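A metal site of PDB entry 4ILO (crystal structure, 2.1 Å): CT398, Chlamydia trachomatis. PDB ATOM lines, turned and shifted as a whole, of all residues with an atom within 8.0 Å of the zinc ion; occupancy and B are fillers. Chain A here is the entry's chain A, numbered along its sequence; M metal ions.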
ATOM      1  N   LYS A 189       6.839   1.234  27.912  1.00  0.00           N
ATOM      2  CA  LYS A 189       7.208   0.180  26.974  1.00  0.00           C
ATOM      3  C   LYS A 189       8.139   0.636  25.867  1.00  0.00           C
ATOM      4  O   LYS A 189       8.878  -0.183  25.319  1.00  0.00           O
ATOM      5  CB  LYS A 189       5.958  -0.392  26.294  1.00  0.00           C
ATOM      6  CG  LYS A 189       4.782  -0.706  27.199  1.00  0.00           C
ATOM      7  CD  LYS A 189       5.049  -1.953  27.983  1.00  0.00           C
ATOM      8  CE  LYS A 189       3.759  -2.538  28.467  1.00  0.00           C
ATOM      9  NZ  LYS A 189       4.052  -3.752  29.230  1.00  0.00           N
ATOM     10  N   VAL A 195      -2.483  -1.177  20.137  1.00  0.00           N
ATOM     11  CA  VAL A 195      -2.118  -2.235  19.186  1.00  0.00           C
ATOM     12  C   VAL A 195      -3.336  -3.065  18.796  1.00  0.00           C
ATOM     13  O   VAL A 195      -4.265  -3.225  19.596  1.00  0.00           O
ATOM     14  CB  VAL A 195      -1.034  -3.177  19.757  1.00  0.00           C
ATOM     15  CG1 VAL A 195       0.269  -2.378  20.090  1.00  0.00           C
ATOM     16  CG2 VAL A 195      -1.583  -3.986  20.959  1.00  0.00           C
ATOM     17  N   VAL A 201      -4.625 -12.870  19.050  1.00  0.00           N
ATOM     18  CA  VAL A 201      -3.695 -12.569  20.149  1.00  0.00           C
ATOM     19  C   VAL A 201      -3.422 -11.055  20.199  1.00  0.00           C
ATOM     20  O   VAL A 201      -3.714 -10.300  19.274  1.00  0.00           O
ATOM     21  CB  VAL A 201      -2.368 -13.374  20.093  1.00  0.00           C
ATOM     22  CG1 VAL A 201      -2.612 -14.815  19.719  1.00  0.00           C
ATOM     23  CG2 VAL A 201      -1.376 -12.755  19.105  1.00  0.00           C
ATOM     24  N   CYS A 202      -2.872 -10.621  21.336  1.00  0.00           N
ATOM     25  CA  CYS A 202      -2.368  -9.255  21.477  1.00  0.00           C
ATOM     26  C   CYS A 202      -1.133  -9.132  20.610  1.00  0.00           C
ATOM     27  O   CYS A 202      -0.209  -9.935  20.732  1.00  0.00           O
ATOM     28  CB  CYS A 202      -2.025  -8.990  22.943  1.00  0.00           C
ATOM     29  SG  CYS A 202      -1.229  -7.411  23.275  1.00  0.00           S
ATOM     30  N   SER A 203      -1.115  -8.147  19.714  1.00  0.00           N
ATOM     31  CA  SER A 203       0.046  -8.015  18.843  1.00  0.00           C
ATOM     32  C   SER A 203       1.201  -7.311  19.532  1.00  0.00           C
ATOM     33  O   SER A 203       2.316  -7.313  19.017  1.00  0.00           O
ATOM     34  CB  SER A 203      -0.344  -7.332  17.528  1.00  0.00           C
ATOM     35  OG  SER A 203      -0.595  -5.966  17.714  1.00  0.00           O
ATOM     36  N   GLY A 204       0.961  -6.730  20.702  1.00  0.00           N
ATOM     37  CA  GLY A 204       2.025  -6.211  21.536  1.00  0.00           C
ATOM     38  C   GLY A 204       2.825  -7.275  22.264  1.00  0.00           C
ATOM     39  O   GLY A 204       4.067  -7.202  22.277  1.00  0.00           O
ATOM     40  N   CYS A 205       2.167  -8.258  22.874  1.00  0.00           N
ATOM     41  CA  CYS A 205       2.861  -9.277  23.665  1.00  0.00           C
ATOM     42  C   CYS A 205       2.689 -10.688  23.126  1.00  0.00           C
ATOM     43  O   CYS A 205       3.404 -11.584  23.573  1.00  0.00           O
ATOM     44  CB  CYS A 205       2.389  -9.214  25.140  1.00  0.00           C
ATOM     45  SG  CYS A 205       0.692  -9.860  25.499  1.00  0.00           S
ATOM     46  N   HIS A 206       1.770 -10.892  22.176  1.00  0.00           N
ATOM     47  CA  HIS A 206       1.486 -12.178  21.513  1.00  0.00           C
ATOM     48  C   HIS A 206       0.745 -13.177  22.390  1.00  0.00           C
ATOM     49  O   HIS A 206       0.696 -14.362  22.092  1.00  0.00           O
ATOM     50  CB  HIS A 206       2.715 -12.808  20.831  1.00  0.00           C
ATOM     51  CG  HIS A 206       3.191 -12.045  19.632  1.00  0.00           C
ATOM     52  ND1 HIS A 206       2.552 -10.901  19.178  1.00  0.00           N
ATOM     53  CD2 HIS A 206       4.224 -12.249  18.798  1.00  0.00           C
ATOM     54  CE1 HIS A 206       3.188 -10.437  18.118  1.00  0.00           C
ATOM     55  NE2 HIS A 206       4.202 -11.243  17.858  1.00  0.00           N
ATOM     56  N   ILE A 207       0.120 -12.734  23.448  1.00  0.00           N
ATOM     57  CA  ILE A 207      -0.671 -13.627  24.284  1.00  0.00           C
ATOM     58  C   ILE A 207      -2.131 -13.591  23.800  1.00  0.00           C
ATOM     59  O   ILE A 207      -2.687 -12.514  23.529  1.00  0.00           O
ATOM     60  CB  ILE A 207      -0.479 -13.267  25.768  1.00  0.00           C
ATOM     61  CG1 ILE A 207       1.023 -13.482  26.136  1.00  0.00           C
ATOM     62  CG2 ILE A 207      -1.412 -14.086  26.687  1.00  0.00           C
ATOM     63  CD1 ILE A 207       1.383 -13.296  27.634  1.00  0.00           C
ATOM     64  N   ALA A 208      -2.727 -14.772  23.620  1.00  0.00           N
ATOM     65  CA  ALA A 208      -4.084 -14.870  23.077  1.00  0.00           C
ATOM     66  C   ALA A 208      -5.128 -14.303  24.041  1.00  0.00           C
ATOM     67  O   ALA A 208      -5.045 -14.463  25.268  1.00  0.00           O
ATOM     68  CB  ALA A 208      -4.428 -16.331  22.773  1.00  0.00           C
ATOM     69  N   LEU A 209      -6.141 -13.649  23.484  1.00  0.00           N
ATOM     70  CA  LEU A 209      -7.240 -13.176  24.316  1.00  0.00           C
ATOM     71  C   LEU A 209      -8.238 -14.303  24.520  1.00  0.00           C
ATOM     72  O   LEU A 209      -8.431 -15.174  23.655  1.00  0.00           O
ATOM     73  CB  LEU A 209      -7.956 -12.034  23.633  1.00  0.00           C
ATOM     74  CG  LEU A 209      -7.279 -10.692  23.450  1.00  0.00           C
ATOM     75  CD1 LEU A 209      -5.950 -10.735  22.593  1.00  0.00           C
ATOM     76  CD2 LEU A 209      -8.321  -9.828  22.782  1.00  0.00           C
ATOM     77  N   PHE A 225      -7.980  -3.160  27.523  1.00  0.00           N
ATOM     78  CA  PHE A 225      -6.545  -3.348  27.689  1.00  0.00           C
ATOM     79  C   PHE A 225      -6.214  -4.835  27.702  1.00  0.00           C
ATOM     80  O   PHE A 225      -7.012  -5.662  28.190  1.00  0.00           O
ATOM     81  CB  PHE A 225      -6.102  -2.769  29.033  1.00  0.00           C
ATOM     82  CG  PHE A 225      -6.569  -1.384  29.230  1.00  0.00           C
ATOM     83  CD1 PHE A 225      -5.939  -0.340  28.583  1.00  0.00           C
ATOM     84  CD2 PHE A 225      -7.680  -1.120  30.031  1.00  0.00           C
ATOM     85  CE1 PHE A 225      -6.364   0.965  28.778  1.00  0.00           C
ATOM     86  CE2 PHE A 225      -8.159   0.181  30.218  1.00  0.00           C
ATOM     87  CZ  PHE A 225      -7.503   1.227  29.591  1.00  0.00           C
ATOM     88  N   CYS A 226      -5.039  -5.179  27.151  1.00  0.00           N
ATOM     89  CA  CYS A 226      -4.562  -6.547  27.213  1.00  0.00           C
ATOM     90  C   CYS A 226      -4.430  -6.974  28.670  1.00  0.00           C
ATOM     91  O   CYS A 226      -3.829  -6.266  29.495  1.00  0.00           O
ATOM     92  CB  CYS A 226      -3.169  -6.642  26.533  1.00  0.00           C
ATOM     93  SG  CYS A 226      -2.497  -8.335  26.522  1.00  0.00           S
ATOM     94  N   GLU A 227      -4.972  -8.163  28.976  1.00  0.00           N
ATOM     95  CA  GLU A 227      -4.958  -8.700  30.330  1.00  0.00           C
ATOM     96  C   GLU A 227      -3.548  -9.084  30.791  1.00  0.00           C
ATOM     97  O   GLU A 227      -3.338  -9.286  31.995  1.00  0.00           O
ATOM     98  CB  GLU A 227      -5.891  -9.895  30.425  1.00  0.00           C
ATOM     99  CG  GLU A 227      -7.374  -9.526  30.298  1.00  0.00           C
ATOM    100  CD  GLU A 227      -8.283 -10.656  30.735  1.00  0.00           C
ATOM    101  OE1 GLU A 227      -8.660 -10.673  31.919  1.00  0.00           O
ATOM    102  OE2 GLU A 227      -8.612 -11.535  29.896  1.00  0.00           O
ATOM    103  N   HIS A 228      -2.577  -9.148  29.872  1.00  0.00           N
ATOM    104  CA  HIS A 228      -1.212  -9.530  30.232  1.00  0.00           C
ATOM    105  C   HIS A 228      -0.192  -8.416  30.141  1.00  0.00           C
ATOM    106  O   HIS A 228       0.646  -8.289  31.036  1.00  0.00           O
ATOM    107  CB  HIS A 228      -0.787 -10.738  29.387  1.00  0.00           C
ATOM    108  CG  HIS A 228      -1.805 -11.842  29.459  1.00  0.00           C
ATOM    109  ND1 HIS A 228      -1.726 -12.892  30.341  1.00  0.00           N
ATOM    110  CD2 HIS A 228      -2.994 -11.981  28.812  1.00  0.00           C
ATOM    111  CE1 HIS A 228      -2.787 -13.667  30.211  1.00  0.00           C
ATOM    112  NE2 HIS A 228      -3.567 -13.146  29.289  1.00  0.00           N
ATOM    113  N   CYS A 229      -0.241  -7.565  29.105  1.00  0.00           N
ATOM    114  CA  CYS A 229       0.743  -6.491  29.008  1.00  0.00           C
ATOM    115  C   CYS A 229       0.165  -5.118  29.293  1.00  0.00           C
ATOM    116  O   CYS A 229       0.931  -4.173  29.408  1.00  0.00           O
ATOM    117  CB  CYS A 229       1.423  -6.502  27.631  1.00  0.00           C
ATOM    118  SG  CYS A 229       0.414  -5.914  26.199  1.00  0.00           S
ATOM    119  N   SER A 230      -1.150  -4.983  29.377  1.00  0.00           N
ATOM    120  CA  SER A 230      -1.847  -3.728  29.729  1.00  0.00           C
ATOM    121  C   SER A 230      -1.914  -2.720  28.561  1.00  0.00           C
ATOM    122  O   SER A 230      -2.483  -1.606  28.766  1.00  0.00           O
ATOM    123  CB  SER A 230      -1.233  -2.990  30.942  1.00  0.00           C
ATOM    124  OG  SER A 230      -1.336  -3.754  32.133  1.00  0.00           O
ATOM    125  N   ARG A 231      -1.379  -3.038  27.385  1.00  0.00           N
ATOM    126  CA  ARG A 231      -1.545  -2.176  26.236  1.00  0.00           C
ATOM    127  C   ARG A 231      -3.029  -2.041  25.868  1.00  0.00           C
ATOM    128  O   ARG A 231      -3.850  -2.918  26.175  1.00  0.00           O
ATOM    129  CB  ARG A 231      -0.816  -2.759  25.034  1.00  0.00           C
ATOM    130  CG  ARG A 231       0.723  -2.753  25.198  1.00  0.00           C
ATOM    131  CD  ARG A 231       1.369  -3.228  23.911  1.00  0.00           C
ATOM    132  NE  ARG A 231       2.798  -2.916  23.858  1.00  0.00           N
ATOM    133  CZ  ARG A 231       3.730  -3.638  24.468  1.00  0.00           C
ATOM    134  NH1 ARG A 231       3.411  -4.693  25.190  1.00  0.00           N
ATOM    135  NH2 ARG A 231       5.014  -3.290  24.346  1.00  0.00           N
ATOM    136  N   ILE A 232      -3.351  -0.958  25.169  1.00  0.00           N
ATOM    137  CA  ILE A 232      -4.719  -0.726  24.648  1.00  0.00           C
ATOM    138  C   ILE A 232      -4.918  -1.569  23.390  1.00  0.00           C
ATOM    139  O   ILE A 232      -4.128  -1.466  22.441  1.00  0.00           O
ATOM    140  CB  ILE A 232      -4.918   0.763  24.320  1.00  0.00           C
ATOM    141  CG1 ILE A 232      -4.881   1.598  25.606  1.00  0.00           C
ATOM    142  CG2 ILE A 232      -6.237   0.973  23.548  1.00  0.00           C
ATOM    143  CD1 ILE A 232      -4.482   3.038  25.397  1.00  0.00           C
ATOM    144  N   LEU A 233      -5.986  -2.361  23.362  1.00  0.00           N
ATOM    145  CA  LEU A 233      -6.293  -3.213  22.214  1.00  0.00           C
ATOM    146  C   LEU A 233      -7.442  -2.613  21.404  1.00  0.00           C
ATOM    147  O   LEU A 233      -8.379  -2.011  21.951  1.00  0.00           O
ATOM    148  CB  LEU A 233      -6.705  -4.616  22.655  1.00  0.00           C
ATOM    149  CG  LEU A 233      -5.720  -5.625  23.261  1.00  0.00           C
ATOM    150  CD1 LEU A 233      -6.469  -6.784  23.879  1.00  0.00           C
ATOM    151  CD2 LEU A 233      -4.719  -6.156  22.178  1.00  0.00           C
HETATM  152 ZN    ZN M   1      -0.518  -7.856  25.410  1.00  0.00          ZN
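The side-chain sulfur (SG) of Cys 202 lies close to the backbone NH (N) of Gly 204 (3.4 Å).
O of Cys 202 lies close to ND1 of His 206.
The backbone NH (N) of Cys 202 sits at hydrogen-bond distance from the backbone carbonyl oxygen (O) of Ile 207 (2.9 Å).
The side-chain sulfur (SG) of Cys 229 lies close to the guanidinium group (NH1) of Arg 231 (3.4 Å).
O of Cys 229 sits at hydrogen-bond distance from NZ of Lys 189 (3.2 Å).
The backbone NH (N) of His 228 sits close to the side-chain sulfur (SG) of Cys 226 (3.4 Å).
The backbone carbonyl oxygen (O) of Arg 231 is in hydrogen-bond range of the backbone NH (N) of Cys 226, at 2.7 Å.
The backbone NH (N) of Ile 207 sits close to the side-chain sulfur (SG) of Cys 205.
Within 4 Å of the zinc ion: Cys 202, Cys 205, Cys 226 and Cys 229.
The zinc ion is bound by SG of Cys 202 (2.3 Å), SG of Cys 229 (2.3 Å), SG of Cys 226 (2.3 Å) and SG of Cys 205 (2.3 Å).
The zinc ion has four donor atoms within binding distance.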
